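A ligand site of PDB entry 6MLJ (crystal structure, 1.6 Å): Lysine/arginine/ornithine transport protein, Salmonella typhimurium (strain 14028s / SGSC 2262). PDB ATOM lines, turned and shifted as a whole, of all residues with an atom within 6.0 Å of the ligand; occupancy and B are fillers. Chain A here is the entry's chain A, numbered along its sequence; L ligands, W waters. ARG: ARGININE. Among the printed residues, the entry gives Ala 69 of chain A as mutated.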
ATOM      1  N   THR A   9      20.890   5.161  36.936  1.00  0.00           N
ATOM      2  CA  THR A   9      20.380   5.827  35.691  1.00  0.00           C
ATOM      3  C   THR A   9      21.592   6.156  34.844  1.00  0.00           C
ATOM      4  O   THR A   9      22.659   6.507  35.434  1.00  0.00           O
ATOM      5  CB  THR A   9      19.486   7.031  36.000  1.00  0.00           C
ATOM      6  OG1 THR A   9      18.757   7.444  34.822  1.00  0.00           O
ATOM      7  CG2 THR A   9      20.214   8.216  36.597  1.00  0.00           C
ATOM      8  N   ASP A  10      21.417   6.108  33.532  1.00  0.00           N
ATOM      9  CA  ASP A  10      22.380   6.525  32.478  1.00  0.00           C
ATOM     10  C   ASP A  10      21.999   7.944  32.090  1.00  0.00           C
ATOM     11  O   ASP A  10      20.962   8.129  31.334  1.00  0.00           O
ATOM     12  CB  ASP A  10      22.305   5.678  31.214  1.00  0.00           C
ATOM     13  CG  ASP A  10      23.181   6.148  30.053  1.00  0.00           C
ATOM     14  OD1 ASP A  10      24.003   7.095  30.227  1.00  0.00           O
ATOM     15  OD2 ASP A  10      23.060   5.520  28.950  1.00  0.00           O
ATOM     16  N   THR A  11      22.830   8.863  32.517  1.00  0.00           N
ATOM     17  CA  THR A  11      22.556  10.324  32.539  1.00  0.00           C
ATOM     18  C   THR A  11      22.850  10.938  31.156  1.00  0.00           C
ATOM     19  O   THR A  11      23.115  12.154  31.120  1.00  0.00           O
ATOM     20  CB  THR A  11      23.371  11.020  33.642  1.00  0.00           C
ATOM     21  OG1 THR A  11      24.733  10.927  33.233  1.00  0.00           O
ATOM     22  CG2 THR A  11      23.047  10.487  35.025  1.00  0.00           C
ATOM     23  N   THR A  12      22.709  10.169  30.039  1.00  0.00           N
ATOM     24  CA  THR A  12      23.011  10.596  28.646  1.00  0.00           C
ATOM     25  C   THR A  12      21.765  10.464  27.729  1.00  0.00           C
ATOM     26  O   THR A  12      21.938  10.355  26.501  1.00  0.00           O
ATOM     27  CB  THR A  12      24.310   9.930  28.166  1.00  0.00           C
ATOM     28  OG1 THR A  12      24.200   8.506  28.088  1.00  0.00           O
ATOM     29  CG2 THR A  12      25.481  10.271  29.074  1.00  0.00           C
ATOM     30  N   TYR A  13      20.549  10.456  28.278  1.00  0.00           N
ATOM     31  CA  TYR A  13      19.325  10.163  27.475  1.00  0.00           C
ATOM     32  C   TYR A  13      18.217  11.184  27.776  1.00  0.00           C
ATOM     33  O   TYR A  13      17.108  10.785  28.235  1.00  0.00           O
ATOM     34  CB  TYR A  13      18.937   8.717  27.770  1.00  0.00           C
ATOM     35  CG  TYR A  13      18.456   7.877  26.619  1.00  0.00           C
ATOM     36  CD1 TYR A  13      17.189   7.312  26.615  1.00  0.00           C
ATOM     37  CD2 TYR A  13      19.263   7.634  25.526  1.00  0.00           C
ATOM     38  CE1 TYR A  13      16.761   6.499  25.580  1.00  0.00           C
ATOM     39  CE2 TYR A  13      18.844   6.825  24.463  1.00  0.00           C
ATOM     40  CZ  TYR A  13      17.594   6.231  24.513  1.00  0.00           C
ATOM     41  OH  TYR A  13      17.136   5.402  23.509  1.00  0.00           O
ATOM     42  N   PHE A  16      14.785  12.054  29.424  1.00  0.00           N
ATOM     43  CA  PHE A  16      14.475  11.086  30.503  1.00  0.00           C
ATOM     44  C   PHE A  16      15.500  11.244  31.648  1.00  0.00           C
ATOM     45  O   PHE A  16      15.058  11.409  32.807  1.00  0.00           O
ATOM     46  CB  PHE A  16      14.357   9.685  29.886  1.00  0.00           C
ATOM     47  CG  PHE A  16      13.297   9.617  28.794  1.00  0.00           C
ATOM     48  CD1 PHE A  16      11.966   9.704  29.158  1.00  0.00           C
ATOM     49  CD2 PHE A  16      13.617   9.517  27.445  1.00  0.00           C
ATOM     50  CE1 PHE A  16      10.964   9.655  28.194  1.00  0.00           C
ATOM     51  CE2 PHE A  16      12.608   9.496  26.482  1.00  0.00           C
ATOM     52  CZ  PHE A  16      11.297   9.528  26.867  1.00  0.00           C
ATOM     53  N   SER A  17      16.787  11.233  31.321  1.00  0.00           N
ATOM     54  CA  SER A  17      17.889  11.308  32.311  1.00  0.00           C
ATOM     55  C   SER A  17      19.135  11.908  31.656  1.00  0.00           C
ATOM     56  O   SER A  17      19.711  11.302  30.728  1.00  0.00           O
ATOM     57  CB  SER A  17      18.150   9.973  32.935  1.00  0.00           C
ATOM     58  OG  SER A  17      19.424  10.042  33.546  1.00  0.00           O
ATOM     59  N   ASP A  29      12.505  10.625  33.979  1.00  0.00           N
ATOM     60  CA  ASP A  29      12.859   9.455  34.855  1.00  0.00           C
ATOM     61  C   ASP A  29      13.177   9.939  36.279  1.00  0.00           C
ATOM     62  O   ASP A  29      12.672   9.337  37.320  1.00  0.00           O
ATOM     63  CB  ASP A  29      14.055   8.676  34.317  1.00  0.00           C
ATOM     64  CG  ASP A  29      13.670   7.664  33.250  1.00  0.00           C
ATOM     65  OD1 ASP A  29      12.413   7.488  33.044  1.00  0.00           O
ATOM     66  OD2 ASP A  29      14.587   7.206  32.525  1.00  0.00           O
ATOM     67  N   PHE A  51      24.751   2.757  30.607  1.00  0.00           N
ATOM     68  CA  PHE A  51      23.543   1.908  30.459  1.00  0.00           C
ATOM     69  C   PHE A  51      23.864   0.422  30.533  1.00  0.00           C
ATOM     70  O   PHE A  51      23.212  -0.316  31.266  1.00  0.00           O
ATOM     71  CB  PHE A  51      22.810   2.354  29.189  1.00  0.00           C
ATOM     72  CG  PHE A  51      21.483   1.680  28.961  1.00  0.00           C
ATOM     73  CD1 PHE A  51      20.380   2.001  29.746  1.00  0.00           C
ATOM     74  CD2 PHE A  51      21.384   0.609  28.084  1.00  0.00           C
ATOM     75  CE1 PHE A  51      19.172   1.342  29.580  1.00  0.00           C
ATOM     76  CE2 PHE A  51      20.183  -0.110  27.976  1.00  0.00           C
ATOM     77  CZ  PHE A  51      19.069   0.308  28.675  1.00  0.00           C
ATOM     78  N   LEU A  54      24.112  -1.089  34.031  1.00  0.00           N
ATOM     79  CA  LEU A  54      23.030  -0.965  35.042  1.00  0.00           C
ATOM     80  C   LEU A  54      22.540  -2.354  35.470  1.00  0.00           C
ATOM     81  O   LEU A  54      22.205  -2.450  36.662  1.00  0.00           O
ATOM     82  CB  LEU A  54      21.873  -0.121  34.489  1.00  0.00           C
ATOM     83  CG  LEU A  54      22.143   1.382  34.280  1.00  0.00           C
ATOM     84  CD1 LEU A  54      21.145   1.981  33.272  1.00  0.00           C
ATOM     85  CD2 LEU A  54      22.049   2.162  35.587  1.00  0.00           C
ATOM     86  N   ILE A  67      16.065   3.201  36.951  1.00  0.00           N
ATOM     87  CA  ILE A  67      15.083   4.028  36.188  1.00  0.00           C
ATOM     88  C   ILE A  67      15.899   4.736  35.091  1.00  0.00           C
ATOM     89  O   ILE A  67      16.656   5.671  35.348  1.00  0.00           O
ATOM     90  CB  ILE A  67      14.303   4.937  37.142  1.00  0.00           C
ATOM     91  CG1 ILE A  67      13.610   4.154  38.237  1.00  0.00           C
ATOM     92  CG2 ILE A  67      13.290   5.703  36.329  1.00  0.00           C
ATOM     93  CD1 ILE A  67      12.982   4.968  39.376  1.00  0.00           C
ATOM     94  N   SER A  68      15.899   4.146  33.905  1.00  0.00           N
ATOM     95  CA  SER A  68      16.785   4.585  32.818  1.00  0.00           C
ATOM     96  C   SER A  68      16.142   4.257  31.500  1.00  0.00           C
ATOM     97  O   SER A  68      16.843   3.770  30.606  1.00  0.00           O
ATOM     98  CB  SER A  68      18.196   4.063  32.879  1.00  0.00           C
ATOM     99  OG  SER A  68      19.080   5.032  32.271  1.00  0.00           O
ATOM    100  N   ALA A  69      14.859   4.669  31.307  1.00  0.00           N
ATOM    101  CA  ALA A  69      14.051   4.306  30.111  1.00  0.00           C
ATOM    102  C   ALA A  69      14.271   2.823  29.773  1.00  0.00           C
ATOM    103  O   ALA A  69      14.650   2.410  28.668  1.00  0.00           O
ATOM    104  CB  ALA A  69      14.384   5.226  28.949  1.00  0.00           C
ATOM    105  N   LEU A  70      14.209   2.018  30.815  1.00  0.00           N
ATOM    106  CA  LEU A  70      14.558   0.594  30.684  1.00  0.00           C
ATOM    107  C   LEU A  70      13.369  -0.155  30.121  1.00  0.00           C
ATOM    108  O   LEU A  70      12.352  -0.448  30.824  1.00  0.00           O
ATOM    109  CB  LEU A  70      14.976   0.047  32.041  1.00  0.00           C
ATOM    110  CG  LEU A  70      15.586  -1.343  32.019  1.00  0.00           C
ATOM    111  CD1 LEU A  70      16.858  -1.452  31.199  1.00  0.00           C
ATOM    112  CD2 LEU A  70      15.796  -1.923  33.422  1.00  0.00           C
ATOM    113  N   SER A  71      13.505  -0.619  28.889  1.00  0.00           N
ATOM    114  CA  SER A  71      12.368  -1.269  28.185  1.00  0.00           C
ATOM    115  C   SER A  71      12.057  -2.605  28.858  1.00  0.00           C
ATOM    116  O   SER A  71      13.037  -3.398  29.148  1.00  0.00           O
ATOM    117  CB  SER A  71      12.732  -1.418  26.717  1.00  0.00           C
ATOM    118  OG  SER A  71      12.596  -0.161  26.018  1.00  0.00           O
ATOM    119  N   ILE A  72      10.789  -2.880  29.091  1.00  0.00           N
ATOM    120  CA  ILE A  72      10.332  -4.176  29.658  1.00  0.00           C
ATOM    121  C   ILE A  72      10.342  -5.269  28.570  1.00  0.00           C
ATOM    122  O   ILE A  72       9.354  -5.346  27.776  1.00  0.00           O
ATOM    123  CB  ILE A  72       8.939  -4.038  30.284  1.00  0.00           C
ATOM    124  CG1 ILE A  72       8.854  -2.821  31.215  1.00  0.00           C
ATOM    125  CG2 ILE A  72       8.522  -5.392  30.878  1.00  0.00           C
ATOM    126  CD1 ILE A  72       7.455  -2.518  31.723  1.00  0.00           C
ATOM    127  N   ARG A  76      14.765  -9.566  29.211  1.00  0.00           N
ATOM    128  CA  ARG A  76      15.199  -8.976  30.505  1.00  0.00           C
ATOM    129  C   ARG A  76      14.376  -9.536  31.650  1.00  0.00           C
ATOM    130  O   ARG A  76      14.924  -9.586  32.773  1.00  0.00           O
ATOM    131  CB  ARG A  76      15.125  -7.450  30.505  1.00  0.00           C
ATOM    132  CG  ARG A  76      16.238  -6.811  29.686  1.00  0.00           C
ATOM    133  CD  ARG A  76      15.930  -5.352  29.369  1.00  0.00           C
ATOM    134  NE  ARG A  76      16.989  -4.748  28.570  1.00  0.00           N
ATOM    135  CZ  ARG A  76      16.897  -3.513  28.040  1.00  0.00           C
ATOM    136  NH1 ARG A  76      15.746  -2.857  28.122  1.00  0.00           N
ATOM    137  NH2 ARG A  76      17.923  -3.002  27.367  1.00  0.00           N
ATOM    138  N   ALA A  89       7.781   3.412  24.672  1.00  0.00           N
ATOM    139  CA  ALA A  89       9.027   3.781  24.010  1.00  0.00           C
ATOM    140  C   ALA A  89       9.211   2.981  22.740  1.00  0.00           C
ATOM    141  O   ALA A  89       9.462   1.776  22.838  1.00  0.00           O
ATOM    142  CB  ALA A  89      10.152   3.544  24.978  1.00  0.00           C
ATOM    143  N   LEU A 116      23.288   2.158  21.084  1.00  0.00           N
ATOM    144  CA  LEU A 116      23.818   2.190  22.476  1.00  0.00           C
ATOM    145  C   LEU A 116      24.199   0.763  22.895  1.00  0.00           C
ATOM    146  O   LEU A 116      23.340  -0.105  22.846  1.00  0.00           O
ATOM    147  CB  LEU A 116      22.733   2.724  23.400  1.00  0.00           C
ATOM    148  CG  LEU A 116      23.090   2.772  24.887  1.00  0.00           C
ATOM    149  CD1 LEU A 116      24.263   3.679  25.147  1.00  0.00           C
ATOM    150  CD2 LEU A 116      21.899   3.234  25.672  1.00  0.00           C
ATOM    151  N   GLY A 118      24.211  -2.343  25.173  1.00  0.00           N
ATOM    152  CA  GLY A 118      23.247  -2.936  26.130  1.00  0.00           C
ATOM    153  C   GLY A 118      21.822  -2.717  25.751  1.00  0.00           C
ATOM    154  O   GLY A 118      20.936  -3.208  26.472  1.00  0.00           O
ATOM    155  N   SER A 119      21.548  -1.884  24.742  1.00  0.00           N
ATOM    156  CA  SER A 119      20.179  -1.440  24.430  1.00  0.00           C
ATOM    157  C   SER A 119      19.439  -2.475  23.584  1.00  0.00           C
ATOM    158  O   SER A 119      20.080  -3.307  22.923  1.00  0.00           O
ATOM    159  CB  SER A 119      20.194  -0.123  23.744  1.00  0.00           C
ATOM    160  OG  SER A 119      20.803  -0.231  22.466  1.00  0.00           O
ATOM    161  N   THR A 120      18.120  -2.393  23.570  1.00  0.00           N
ATOM    162  CA  THR A 120      17.216  -3.125  22.636  1.00  0.00           C
ATOM    163  C   THR A 120      17.624  -2.810  21.198  1.00  0.00           C
ATOM    164  O   THR A 120      17.683  -3.706  20.384  1.00  0.00           O
ATOM    165  CB  THR A 120      15.750  -2.803  22.955  1.00  0.00           C
ATOM    166  OG1 THR A 120      15.459  -1.395  22.838  1.00  0.00           O
ATOM    167  CG2 THR A 120      15.399  -3.326  24.320  1.00  0.00           C
ATOM    168  N   GLN A 121      17.887  -1.535  20.916  1.00  0.00           N
ATOM    169  CA  GLN A 121      18.344  -1.107  19.561  1.00  0.00           C
ATOM    170  C   GLN A 121      19.604  -1.828  19.136  1.00  0.00           C
ATOM    171  O   GLN A 121      19.722  -2.143  17.896  1.00  0.00           O
ATOM    172  CB  GLN A 121      18.433   0.418  19.444  1.00  0.00           C
ATOM    173  CG  GLN A 121      17.101   1.150  19.678  1.00  0.00           C
ATOM    174  CD  GLN A 121      16.877   1.408  21.142  1.00  0.00           C
ATOM    175  OE1 GLN A 121      17.796   1.201  21.963  1.00  0.00           O
ATOM    176  NE2 GLN A 121      15.720   1.886  21.517  1.00  0.00           N
ATOM    177  N   GLN A 142      24.866   7.541  24.688  1.00  0.00           N
ATOM    178  CA  GLN A 142      24.077   8.085  23.528  1.00  0.00           C
ATOM    179  C   GLN A 142      24.693   9.428  23.113  1.00  0.00           C
ATOM    180  O   GLN A 142      24.627   9.772  21.929  1.00  0.00           O
ATOM    181  CB  GLN A 142      22.603   8.127  23.893  1.00  0.00           C
ATOM    182  CG  GLN A 142      21.691   8.557  22.754  1.00  0.00           C
ATOM    183  CD  GLN A 142      21.604   7.594  21.567  1.00  0.00           C
ATOM    184  OE1 GLN A 142      21.535   6.370  21.697  1.00  0.00           O
ATOM    185  NE2 GLN A 142      21.473   8.178  20.371  1.00  0.00           N
ATOM    186  N   ASP A 160      15.590   5.307  21.114  1.00  0.00           N
ATOM    187  CA  ASP A 160      14.184   5.633  21.453  1.00  0.00           C
ATOM    188  C   ASP A 160      13.756   6.884  20.658  1.00  0.00           C
ATOM    189  O   ASP A 160      14.518   7.894  20.640  1.00  0.00           O
ATOM    190  CB  ASP A 160      14.014   5.725  22.987  1.00  0.00           C
ATOM    191  CG  ASP A 160      14.122   4.360  23.696  1.00  0.00           C
ATOM    192  OD1 ASP A 160      14.151   3.293  22.977  1.00  0.00           O
ATOM    193  OD2 ASP A 160      14.088   4.330  24.972  1.00  0.00           O
ATOM    194  N   THR A 194       8.648   1.084  29.293  1.00  0.00           N
ATOM    195  CA  THR A 194       9.767   1.143  30.265  1.00  0.00           C
ATOM    196  C   THR A 194       9.197   0.898  31.648  1.00  0.00           C
ATOM    197  O   THR A 194       7.991   1.065  31.831  1.00  0.00           O
ATOM    198  CB  THR A 194      10.515   2.470  30.093  1.00  0.00           C
ATOM    199  OG1 THR A 194       9.695   3.440  30.713  1.00  0.00           O
ATOM    200  CG2 THR A 194      10.993   2.697  28.677  1.00  0.00           C
HETATM  201  N   ARG L   1      14.787   1.671  25.814  1.00  0.00           N
HETATM  202  CA  ARG L   1      16.044   1.230  25.285  1.00  0.00           C
HETATM  203  C   ARG L   1      16.402  -0.008  26.101  1.00  0.00           C
HETATM  204  O   ARG L   1      15.638  -0.274  27.134  1.00  0.00           O
HETATM  205  CB  ARG L   1      17.149   2.317  25.314  1.00  0.00           C
HETATM  206  CG  ARG L   1      17.236   3.158  26.613  1.00  0.00           C
HETATM  207  CD  ARG L   1      18.562   3.853  27.118  1.00  0.00           C
HETATM  208  NE  ARG L   1      18.381   4.686  28.319  1.00  0.00           N
HETATM  209  CZ  ARG L   1      19.272   5.508  28.890  1.00  0.00           C
HETATM  210  NH1 ARG L   1      20.477   5.665  28.357  1.00  0.00           N
HETATM  211  NH2 ARG L   1      18.956   6.218  29.979  1.00  0.00           N
HETATM  212  OXT ARG L   1      17.365  -0.655  25.790  1.00  0.00           O
HETATM  213  O   HOH W   1      16.634   7.450  30.571  1.00  0.00           O
HETATM  214  O   HOH W   2      23.067   6.694  26.593  1.00  0.00           O
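Water W1 lies within hydrogen-bond range of a nitrogen (NH2) of the ligand (2.7 Å), the side-chain carboxylate (OD2) of Asp 29 (2.8 Å) and the backbone NH (N) of Ala 69 (3.4 Å).
Water W2 lies within hydrogen-bond range of the side-chain hydroxyl (OG1) of Thr 12 (2.6 Å), the side-chain carboxylate (OD2) of Asp 10 (2.6 Å), the backbone NH (N) of Gln 142 (2.8 Å) and a nitrogen (NH1) of the ligand (3.3 Å).
O of Ser 68 is in hydrogen-bond range of NE of the ligand (2.9 Å).
A nitrogen (NH2) of the ligand sits at hydrogen-bond distance from the side-chain hydroxyl (OG) of Ser 68 (2.6 Å).
O of Asp 10 lies within hydrogen-bond range of NH2 of the ligand (3.1 Å).
A nitrogen (NH1) of the ligand is in salt-bridge range of the side-chain carboxylate (OD2) of Asp 10, at 2.7 Å.
The guanidinium group of Arg 76 lies within salt-bridge range of an oxygen (O) of the ligand (2.8 Å).
N of Ser 71 lies within hydrogen-bond range of O of the ligand.
N of the ligand lies within hydrogen-bond range of OG of Ser 71 (2.9 Å).
A nitrogen (N) of the ligand lies within salt-bridge range of the side-chain carboxylate (OD2) of Asp 160 (2.9 Å).
The backbone NH of Thr 120 sits at hydrogen-bond distance from an oxygen (OXT) of the ligand (2.9 Å).
The backbone carbonyl oxygen (O) of Ala 69 sits at hydrogen-bond distance from a nitrogen (N) of the ligand.
The side-chain hydroxyl (OG) of Ser 68 is in hydrogen-bond range of the backbone NH (N) of Asp 10, 2.9 Å away.
The side-chain hydroxyl (OG1) of Thr 12 lies within hydrogen-bond range of the side-chain carboxylate (OD1) of Asp 10 (2.6 Å).
The backbone carbonyl oxygen (O) of Asp 10 lies within hydrogen-bond range of the side-chain hydroxyl (OG) of Ser 17 (3.3 Å).
NH2 of Arg 76 sits at hydrogen-bond distance from O of Gly 118, 3.1 Å away.
The backbone NH (N) of Asp 160 lies within hydrogen-bond range of the side-chain hydroxyl (OH) of Tyr 13 (2.9 Å).
The backbone NH of Ala 69 sits at hydrogen-bond distance from the side-chain carboxylate of Asp 29 (2.8 Å).
The side-chain hydroxyl (OG) of Ser 119 sits close to the side-chain amide oxygen (OE1) of Gln 121 (3.4 Å).
The side-chain hydroxyl (OG) of Ser 119 sits at hydrogen-bond distance from the backbone carbonyl oxygen (O) of Leu 116 (2.6 Å).
Merely in contact with the ligand: Ser 119 (3.2 Å), Tyr 13 (3.3 Å), Phe 51 (3.5 Å), Gln 121 (3.6 Å), Leu 116 (3.7 Å) and Leu 70 (3.8 Å).
Hydrophobic or aromatic side chains that line the ligand: Tyr 13, Phe 51 and Leu 116.
13 residues have an atom within 4 Å of the ligand: Asp 10, Tyr 13, Phe 51, Ser 68, Ala 69, Leu 70, Ser 71, Arg 76, Leu 116, Ser 119, Thr 120, Gln 121 and Asp 160.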
